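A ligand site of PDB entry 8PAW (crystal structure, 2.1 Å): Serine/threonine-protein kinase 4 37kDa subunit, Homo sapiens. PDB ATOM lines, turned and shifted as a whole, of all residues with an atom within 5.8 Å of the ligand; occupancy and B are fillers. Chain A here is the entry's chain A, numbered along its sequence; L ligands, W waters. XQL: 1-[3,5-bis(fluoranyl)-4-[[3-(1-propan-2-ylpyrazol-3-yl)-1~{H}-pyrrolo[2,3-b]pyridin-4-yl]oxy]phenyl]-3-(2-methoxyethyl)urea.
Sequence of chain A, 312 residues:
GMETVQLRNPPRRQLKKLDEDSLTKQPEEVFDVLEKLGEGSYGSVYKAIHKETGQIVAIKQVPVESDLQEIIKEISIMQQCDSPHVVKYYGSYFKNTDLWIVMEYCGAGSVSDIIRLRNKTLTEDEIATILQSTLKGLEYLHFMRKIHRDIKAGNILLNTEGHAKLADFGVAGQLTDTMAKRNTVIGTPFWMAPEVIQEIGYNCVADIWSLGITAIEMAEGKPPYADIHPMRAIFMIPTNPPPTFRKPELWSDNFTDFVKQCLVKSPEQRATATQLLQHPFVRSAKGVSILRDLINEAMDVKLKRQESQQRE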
ATOM      1  N   LEU A  37      -1.783  -8.332 -19.957  1.00  0.00           N
ATOM      2  CA  LEU A  37      -0.659  -9.189 -20.437  1.00  0.00           C
ATOM      3  C   LEU A  37       0.659  -8.421 -20.331  1.00  0.00           C
ATOM      4  O   LEU A  37       1.699  -9.066 -20.326  1.00  0.00           O
ATOM      5  CB  LEU A  37      -0.898  -9.575 -21.898  1.00  0.00           C
ATOM      6  CG  LEU A  37      -2.092 -10.482 -22.173  1.00  0.00           C
ATOM      7  CD1 LEU A  37      -2.306 -10.635 -23.663  1.00  0.00           C
ATOM      8  CD2 LEU A  37      -1.898 -11.835 -21.512  1.00  0.00           C
ATOM      9  N   GLY A  38       0.606  -7.084 -20.275  1.00  0.00           N
ATOM     10  CA  GLY A  38       1.807  -6.241 -20.285  1.00  0.00           C
ATOM     11  C   GLY A  38       1.525  -4.810 -19.876  1.00  0.00           C
ATOM     12  O   GLY A  38       0.373  -4.374 -20.034  1.00  0.00           O
ATOM     13  N   GLU A  39       2.548  -4.148 -19.341  1.00  0.00           N
ATOM     14  CA  GLU A  39       2.641  -2.685 -19.082  1.00  0.00           C
ATOM     15  C   GLU A  39       4.053  -2.288 -19.552  1.00  0.00           C
ATOM     16  O   GLU A  39       4.435  -1.135 -19.336  1.00  0.00           O
ATOM     17  CB  GLU A  39       2.350  -2.388 -17.608  1.00  0.00           C
ATOM     18  CG  GLU A  39       0.960  -1.784 -17.335  1.00  0.00           C
ATOM     19  CD  GLU A  39       0.884  -0.263 -17.325  1.00  0.00           C
ATOM     20  OE1 GLU A  39       1.355   0.346 -16.338  1.00  0.00           O
ATOM     21  OE2 GLU A  39       0.334   0.326 -18.291  1.00  0.00           O
ATOM     22  N   VAL A  45      -1.438  -3.697 -22.415  1.00  0.00           N
ATOM     23  CA  VAL A  45      -1.932  -4.774 -23.320  1.00  0.00           C
ATOM     24  C   VAL A  45      -2.770  -5.770 -22.519  1.00  0.00           C
ATOM     25  O   VAL A  45      -2.333  -6.156 -21.418  1.00  0.00           O
ATOM     26  CB  VAL A  45      -0.767  -5.467 -24.017  1.00  0.00           C
ATOM     27  CG1 VAL A  45      -1.259  -6.515 -25.008  1.00  0.00           C
ATOM     28  CG2 VAL A  45       0.144  -4.461 -24.703  1.00  0.00           C
ATOM     29  N   ALA A  58      -5.391 -10.085 -28.450  1.00  0.00           N
ATOM     30  CA  ALA A  58      -4.626  -9.113 -27.644  1.00  0.00           C
ATOM     31  C   ALA A  58      -5.117  -7.710 -28.031  1.00  0.00           C
ATOM     32  O   ALA A  58      -5.297  -7.456 -29.242  1.00  0.00           O
ATOM     33  CB  ALA A  58      -3.137  -9.286 -27.861  1.00  0.00           C
ATOM     34  N   LYS A  60      -4.150  -3.713 -27.336  1.00  0.00           N
ATOM     35  CA  LYS A  60      -3.244  -2.685 -26.793  1.00  0.00           C
ATOM     36  C   LYS A  60      -4.077  -1.403 -26.631  1.00  0.00           C
ATOM     37  O   LYS A  60      -4.712  -1.006 -27.619  1.00  0.00           O
ATOM     38  CB  LYS A  60      -2.036  -2.495 -27.718  1.00  0.00           C
ATOM     39  CG  LYS A  60      -0.993  -1.517 -27.228  1.00  0.00           C
ATOM     40  CD  LYS A  60       0.171  -1.442 -28.157  1.00  0.00           C
ATOM     41  CE  LYS A  60       0.988  -0.184 -27.961  1.00  0.00           C
ATOM     42  NZ  LYS A  60       1.806  -0.254 -26.732  1.00  0.00           N
ATOM     43  N   GLU A  74       3.325   1.534 -37.080  1.00  0.00           N
ATOM     44  CA  GLU A  74       3.219   0.089 -36.784  1.00  0.00           C
ATOM     45  C   GLU A  74       1.924  -0.464 -37.402  1.00  0.00           C
ATOM     46  O   GLU A  74       1.956  -1.507 -38.092  1.00  0.00           O
ATOM     47  CB  GLU A  74       3.293  -0.019 -35.259  1.00  0.00           C
ATOM     48  CG  GLU A  74       2.627  -1.231 -34.670  1.00  0.00           C
ATOM     49  CD  GLU A  74       3.512  -1.884 -33.623  1.00  0.00           C
ATOM     50  OE1 GLU A  74       3.808  -3.118 -33.851  1.00  0.00           O
ATOM     51  OE2 GLU A  74       3.969  -1.113 -32.676  1.00  0.00           O
ATOM     52  N   MET A  78       1.405  -3.375 -40.386  1.00  0.00           N
ATOM     53  CA  MET A  78       0.697  -4.645 -40.066  1.00  0.00           C
ATOM     54  C   MET A  78      -0.553  -4.765 -40.946  1.00  0.00           C
ATOM     55  O   MET A  78      -0.857  -5.924 -41.355  1.00  0.00           O
ATOM     56  CB  MET A  78       0.267  -4.748 -38.602  1.00  0.00           C
ATOM     57  CG  MET A  78       1.398  -5.166 -37.659  1.00  0.00           C
ATOM     58  SD  MET A  78       0.802  -5.370 -35.947  1.00  0.00           S
ATOM     59  CE  MET A  78       0.705  -3.642 -35.525  1.00  0.00           C
ATOM     60  N   VAL A  87       2.440 -11.043 -36.857  1.00  0.00           N
ATOM     61  CA  VAL A  87       1.281 -10.754 -35.942  1.00  0.00           C
ATOM     62  C   VAL A  87       0.240  -9.965 -36.737  1.00  0.00           C
ATOM     63  O   VAL A  87       0.597  -8.965 -37.350  1.00  0.00           O
ATOM     64  CB  VAL A  87       1.703 -10.044 -34.646  1.00  0.00           C
ATOM     65  CG1 VAL A  87       0.505  -9.677 -33.773  1.00  0.00           C
ATOM     66  CG2 VAL A  87       2.651 -10.882 -33.831  1.00  0.00           C
ATOM     67  N   ILE A 101      -6.245  -1.126 -29.912  1.00  0.00           N
ATOM     68  CA  ILE A 101      -5.607  -1.762 -31.096  1.00  0.00           C
ATOM     69  C   ILE A 101      -5.712  -3.273 -30.918  1.00  0.00           C
ATOM     70  O   ILE A 101      -5.014  -3.806 -30.040  1.00  0.00           O
ATOM     71  CB  ILE A 101      -4.147  -1.311 -31.229  1.00  0.00           C
ATOM     72  CG1 ILE A 101      -4.040   0.218 -31.316  1.00  0.00           C
ATOM     73  CG2 ILE A 101      -3.476  -2.022 -32.388  1.00  0.00           C
ATOM     74  CD1 ILE A 101      -2.924   0.818 -30.475  1.00  0.00           C
ATOM     75  N   MET A 103      -5.308  -7.203 -31.979  1.00  0.00           N
ATOM     76  CA  MET A 103      -4.236  -7.986 -32.654  1.00  0.00           C
ATOM     77  C   MET A 103      -4.362  -9.474 -32.331  1.00  0.00           C
ATOM     78  O   MET A 103      -5.047  -9.838 -31.346  1.00  0.00           O
ATOM     79  CB  MET A 103      -2.868  -7.498 -32.204  1.00  0.00           C
ATOM     80  CG  MET A 103      -2.559  -6.072 -32.652  1.00  0.00           C
ATOM     81  SD  MET A 103      -0.945  -5.498 -32.030  1.00  0.00           S
ATOM     82  CE  MET A 103      -1.336  -5.192 -30.308  1.00  0.00           C
ATOM     83  N   GLU A 104      -3.643 -10.292 -33.107  1.00  0.00           N
ATOM     84  CA  GLU A 104      -3.533 -11.761 -32.933  1.00  0.00           C
ATOM     85  C   GLU A 104      -2.889 -12.034 -31.576  1.00  0.00           C
ATOM     86  O   GLU A 104      -1.853 -11.385 -31.277  1.00  0.00           O
ATOM     87  CB  GLU A 104      -2.745 -12.336 -34.097  1.00  0.00           C
ATOM     88  CG  GLU A 104      -2.472 -13.825 -34.010  1.00  0.00           C
ATOM     89  CD  GLU A 104      -1.652 -14.314 -35.194  1.00  0.00           C
ATOM     90  OE1 GLU A 104      -1.138 -13.459 -35.985  1.00  0.00           O
ATOM     91  OE2 GLU A 104      -1.528 -15.520 -35.325  1.00  0.00           O
ATOM     92  N   TYR A 105      -3.487 -12.929 -30.781  1.00  0.00           N
ATOM     93  CA  TYR A 105      -2.999 -13.359 -29.455  1.00  0.00           C
ATOM     94  C   TYR A 105      -1.839 -14.366 -29.611  1.00  0.00           C
ATOM     95  O   TYR A 105      -1.988 -15.398 -30.309  1.00  0.00           O
ATOM     96  CB  TYR A 105      -4.145 -13.970 -28.643  1.00  0.00           C
ATOM     97  CG  TYR A 105      -3.747 -14.500 -27.286  1.00  0.00           C
ATOM     98  CD1 TYR A 105      -3.228 -13.641 -26.327  1.00  0.00           C
ATOM     99  CD2 TYR A 105      -3.890 -15.835 -26.959  1.00  0.00           C
ATOM    100  CE1 TYR A 105      -2.884 -14.099 -25.064  1.00  0.00           C
ATOM    101  CE2 TYR A 105      -3.548 -16.317 -25.698  1.00  0.00           C
ATOM    102  CZ  TYR A 105      -3.050 -15.438 -24.753  1.00  0.00           C
ATOM    103  OH  TYR A 105      -2.694 -15.866 -23.515  1.00  0.00           O
ATOM    104  N   CYS A 106      -0.696 -14.070 -28.989  1.00  0.00           N
ATOM    105  CA  CYS A 106       0.493 -14.955 -28.963  1.00  0.00           C
ATOM    106  C   CYS A 106       0.782 -15.303 -27.495  1.00  0.00           C
ATOM    107  O   CYS A 106       1.528 -14.564 -26.842  1.00  0.00           O
ATOM    108  CB  CYS A 106       1.678 -14.297 -29.671  1.00  0.00           C
ATOM    109  SG  CYS A 106       1.374 -13.965 -31.420  1.00  0.00           S
ATOM    110  N   GLY A 107       0.172 -16.378 -26.999  1.00  0.00           N
ATOM    111  CA  GLY A 107       0.005 -16.647 -25.558  1.00  0.00           C
ATOM    112  C   GLY A 107       1.296 -16.983 -24.837  1.00  0.00           C
ATOM    113  O   GLY A 107       1.326 -16.823 -23.610  1.00  0.00           O
ATOM    114  N   GLY A 109       4.052 -15.316 -25.209  1.00  0.00           N
ATOM    115  CA  GLY A 109       4.823 -14.058 -25.171  1.00  0.00           C
ATOM    116  C   GLY A 109       6.063 -14.159 -26.056  1.00  0.00           C
ATOM    117  O   GLY A 109       6.061 -14.946 -27.018  1.00  0.00           O
ATOM    118  N   SER A 110       7.093 -13.381 -25.761  1.00  0.00           N
ATOM    119  CA  SER A 110       8.279 -13.230 -26.644  1.00  0.00           C
ATOM    120  C   SER A 110       9.283 -14.371 -26.371  1.00  0.00           C
ATOM    121  O   SER A 110       9.224 -15.031 -25.311  1.00  0.00           O
ATOM    122  CB  SER A 110       8.913 -11.886 -26.464  1.00  0.00           C
ATOM    123  OG  SER A 110       9.597 -11.796 -25.218  1.00  0.00           O
ATOM    124  N   ASP A 113      11.062 -13.325 -23.202  1.00  0.00           N
ATOM    125  CA  ASP A 113      10.199 -13.726 -22.057  1.00  0.00           C
ATOM    126  C   ASP A 113      10.417 -15.209 -21.723  1.00  0.00           C
ATOM    127  O   ASP A 113      10.618 -15.523 -20.548  1.00  0.00           O
ATOM    128  CB  ASP A 113       8.700 -13.541 -22.323  1.00  0.00           C
ATOM    129  CG  ASP A 113       8.224 -12.104 -22.432  1.00  0.00           C
ATOM    130  OD1 ASP A 113       8.867 -11.229 -21.810  1.00  0.00           O
ATOM    131  OD2 ASP A 113       7.190 -11.883 -23.121  1.00  0.00           O
ATOM    132  N   ARG A 116      13.883 -15.836 -20.098  1.00  0.00           N
ATOM    133  CA  ARG A 116      13.885 -15.280 -18.713  1.00  0.00           C
ATOM    134  C   ARG A 116      13.026 -16.164 -17.791  1.00  0.00           C
ATOM    135  O   ARG A 116      13.499 -16.473 -16.701  1.00  0.00           O
ATOM    136  CB  ARG A 116      13.424 -13.815 -18.717  1.00  0.00           C
ATOM    137  CG  ARG A 116      13.384 -13.207 -17.325  1.00  0.00           C
ATOM    138  CD  ARG A 116      12.959 -11.756 -17.264  1.00  0.00           C
ATOM    139  NE  ARG A 116      11.894 -11.403 -18.193  1.00  0.00           N
ATOM    140  CZ  ARG A 116      10.627 -11.856 -18.131  1.00  0.00           C
ATOM    141  NH1 ARG A 116      10.249 -12.701 -17.189  1.00  0.00           N
ATOM    142  NH2 ARG A 116       9.742 -11.470 -19.038  1.00  0.00           N
ATOM    143  N   LEU A 157       7.264 -13.301 -31.206  1.00  0.00           N
ATOM    144  CA  LEU A 157       6.249 -13.844 -30.276  1.00  0.00           C
ATOM    145  C   LEU A 157       5.920 -15.279 -30.670  1.00  0.00           C
ATOM    146  O   LEU A 157       5.970 -15.592 -31.865  1.00  0.00           O
ATOM    147  CB  LEU A 157       4.988 -12.968 -30.324  1.00  0.00           C
ATOM    148  CG  LEU A 157       5.207 -11.471 -30.115  1.00  0.00           C
ATOM    149  CD1 LEU A 157       3.867 -10.771 -29.963  1.00  0.00           C
ATOM    150  CD2 LEU A 157       6.114 -11.224 -28.917  1.00  0.00           C
ATOM    151  N   ALA A 167       6.755  -9.172 -34.530  1.00  0.00           N
ATOM    152  CA  ALA A 167       5.989  -8.095 -33.862  1.00  0.00           C
ATOM    153  C   ALA A 167       6.869  -6.843 -33.802  1.00  0.00           C
ATOM    154  O   ALA A 167       8.095  -6.927 -34.082  1.00  0.00           O
ATOM    155  CB  ALA A 167       5.543  -8.559 -32.481  1.00  0.00           C
ATOM    156  N   ASP A 168       6.255  -5.715 -33.445  1.00  0.00           N
ATOM    157  CA  ASP A 168       6.884  -4.389 -33.241  1.00  0.00           C
ATOM    158  C   ASP A 168       7.443  -3.871 -34.562  1.00  0.00           C
ATOM    159  O   ASP A 168       8.695  -3.893 -34.750  1.00  0.00           O
ATOM    160  CB  ASP A 168       7.941  -4.406 -32.139  1.00  0.00           C
ATOM    161  CG  ASP A 168       8.397  -3.005 -31.717  1.00  0.00           C
ATOM    162  OD1 ASP A 168       7.981  -2.010 -32.384  1.00  0.00           O
ATOM    163  OD2 ASP A 168       9.214  -2.909 -30.768  1.00  0.00           O
ATOM    164  N   PHE A 169       6.555  -3.313 -35.380  1.00  0.00           N
ATOM    165  CA  PHE A 169       6.852  -2.618 -36.658  1.00  0.00           C
ATOM    166  C   PHE A 169       7.019  -1.120 -36.427  1.00  0.00           C
ATOM    167  O   PHE A 169       6.961  -0.369 -37.410  1.00  0.00           O
ATOM    168  CB  PHE A 169       5.761  -3.004 -37.669  1.00  0.00           C
ATOM    169  CG  PHE A 169       5.873  -4.434 -38.113  1.00  0.00           C
ATOM    170  CD1 PHE A 169       5.269  -5.451 -37.396  1.00  0.00           C
ATOM    171  CD2 PHE A 169       6.663  -4.775 -39.200  1.00  0.00           C
ATOM    172  CE1 PHE A 169       5.417  -6.779 -37.783  1.00  0.00           C
ATOM    173  CE2 PHE A 169       6.796  -6.096 -39.605  1.00  0.00           C
ATOM    174  CZ  PHE A 169       6.186  -7.100 -38.883  1.00  0.00           C
HETATM  175  C5  XQL L   1       0.163 -10.259 -28.509  1.00  0.00           C
HETATM  176  C7  XQL L   1       0.321 -11.591 -26.587  1.00  0.00           C
HETATM  177  C8  XQL L   1       1.093 -10.636 -25.958  1.00  0.00           C
HETATM  178  C15 XQL L   1       4.855  -9.375 -23.017  1.00  0.00           C
HETATM  179  C17 XQL L   1       6.115  -9.015 -21.030  1.00  0.00           C
HETATM  180  C20 XQL L   1       8.472  -7.761 -19.438  1.00  0.00           C
HETATM  181  C22 XQL L   1       9.290  -7.257 -17.219  1.00  0.00           C
HETATM  182  C24 XQL L   1       3.798  -8.511 -22.755  1.00  0.00           C
HETATM  183  C33 XQL L   1       1.887  -2.943 -30.798  1.00  0.00           C
HETATM  184  C32 XQL L   1       2.900  -3.623 -29.861  1.00  0.00           C
HETATM  185  C34 XQL L   1       4.295  -3.641 -30.446  1.00  0.00           C
HETATM  186  N29 XQL L   1       2.415  -4.931 -29.275  1.00  0.00           N
HETATM  187  N28 XQL L   1       1.950  -5.973 -29.813  1.00  0.00           N
HETATM  188  C30 XQL L   1       2.440  -5.069 -27.967  1.00  0.00           C
HETATM  189  C31 XQL L   1       1.964  -6.289 -27.702  1.00  0.00           C
HETATM  190  C27 XQL L   1       1.664  -6.914 -28.848  1.00  0.00           C
HETATM  191  C2  XQL L   1       1.040  -8.203 -28.935  1.00  0.00           C
HETATM  192  C1  XQL L   1       0.926  -9.223 -27.942  1.00  0.00           C
HETATM  193  C3  XQL L   1       0.331  -8.653 -29.969  1.00  0.00           C
HETATM  194  N4  XQL L   1      -0.170  -9.871 -29.743  1.00  0.00           N
HETATM  195  N6  XQL L   1      -0.110 -11.409 -27.821  1.00  0.00           N
HETATM  196  C9  XQL L   1       1.393  -9.432 -26.625  1.00  0.00           C
HETATM  197  O10 XQL L   1       2.140  -8.448 -26.020  1.00  0.00           O
HETATM  198  C11 XQL L   1       3.026  -8.758 -25.026  1.00  0.00           C
HETATM  199  C25 XQL L   1       2.889  -8.206 -23.766  1.00  0.00           C
HETATM  200  F26 XQL L   1       1.840  -7.401 -23.534  1.00  0.00           F
HETATM  201  C12 XQL L   1       4.076  -9.606 -25.270  1.00  0.00           C
HETATM  202  F13 XQL L   1       4.191 -10.082 -26.498  1.00  0.00           F
HETATM  203  C14 XQL L   1       4.996  -9.905 -24.289  1.00  0.00           C
HETATM  204  N16 XQL L   1       5.762  -9.725 -22.114  1.00  0.00           N
HETATM  205  O23 XQL L   1       5.576  -7.969 -20.692  1.00  0.00           O
HETATM  206  N18 XQL L   1       7.062  -9.558 -20.273  1.00  0.00           N
HETATM  207  C19 XQL L   1       7.551  -8.923 -19.048  1.00  0.00           C
HETATM  208  O21 XQL L   1       9.589  -7.767 -18.556  1.00  0.00           O
HETATM  209  O   HOH W   1       4.810  -5.851 -18.923  1.00  0.00           O
HETATM  210  O   HOH W   2       3.363  -2.782 -26.706  1.00  0.00           O
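A nitrogen (N6) of the ligand is in hydrogen-bond range of the backbone NH of Cys 106.
The side-chain carboxylate (OD2) of Asp 113 lies within hydrogen-bond range of a nitrogen (N16) of the ligand, at 2.8 Å.
O of Glu 104 lies within hydrogen-bond range of N4 of the ligand (2.7 Å).
The backbone NH of Ile 101 lies within hydrogen-bond range of the backbone carbonyl oxygen of Lys 60 (2.8 Å).
O of Gly 38 lies within hydrogen-bond range of N of Val 45 (3.1 Å).
O of Ala 58 is in hydrogen-bond range of N of Met 103, at 2.7 Å.
The backbone NH (N) of Leu 37 lies within hydrogen-bond range of the backbone carbonyl oxygen (O) of Val 45, at 2.7 Å.
OG of Ser 110 lies within hydrogen-bond range of N of Asp 113, at 2.9 Å.
The side-chain carboxylate of Glu 74 sits at hydrogen-bond distance from the backbone NH of Phe 169 (3.1 Å).
OD1 of Asp 113 lies within salt-bridge range of NH2 of Arg 116.
The backbone NH (N) of Gly 38 lies close to a fluorine (F26) of the ligand, 3.5 Å away.
N28 of the ligand sits close to SD of Met 103 (3.7 Å).
Residues that only touch the ligand: Leu 37 (3.3 Å), Val 45 (3.3 Å), Leu 157 (3.3 Å), Glu 74 (3.3 Å), Arg 116 (3.4 Å), Lys 60 (3.5 Å), Ala 58 (3.5 Å), Tyr 105 (3.8 Å), Asp 168 (3.9 Å) and Val 87 (3.9 Å).
Hydrophobic or aromatic side chains within 4 Å of the ligand: Leu 37, Val 45, Ala 58, Val 87, Met 103 and Leu 157.
Within 4 Å of the ligand: Leu 37, Gly 38, Val 45, Ala 58, Lys 60, Glu 74, Val 87, Met 103, Glu 104, Tyr 105, Cys 106, Asp 113, Arg 116, Leu 157 and Asp 168.
Along chain A the residues within 4 Å of the ligand span positions 37 to 168.
The nearest printed residue that does not touch the ligand is Gly 109 (4.2 Å).
Water W1 bridges the backbone NH of Glu 39 and an oxygen (O23) of the ligand.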
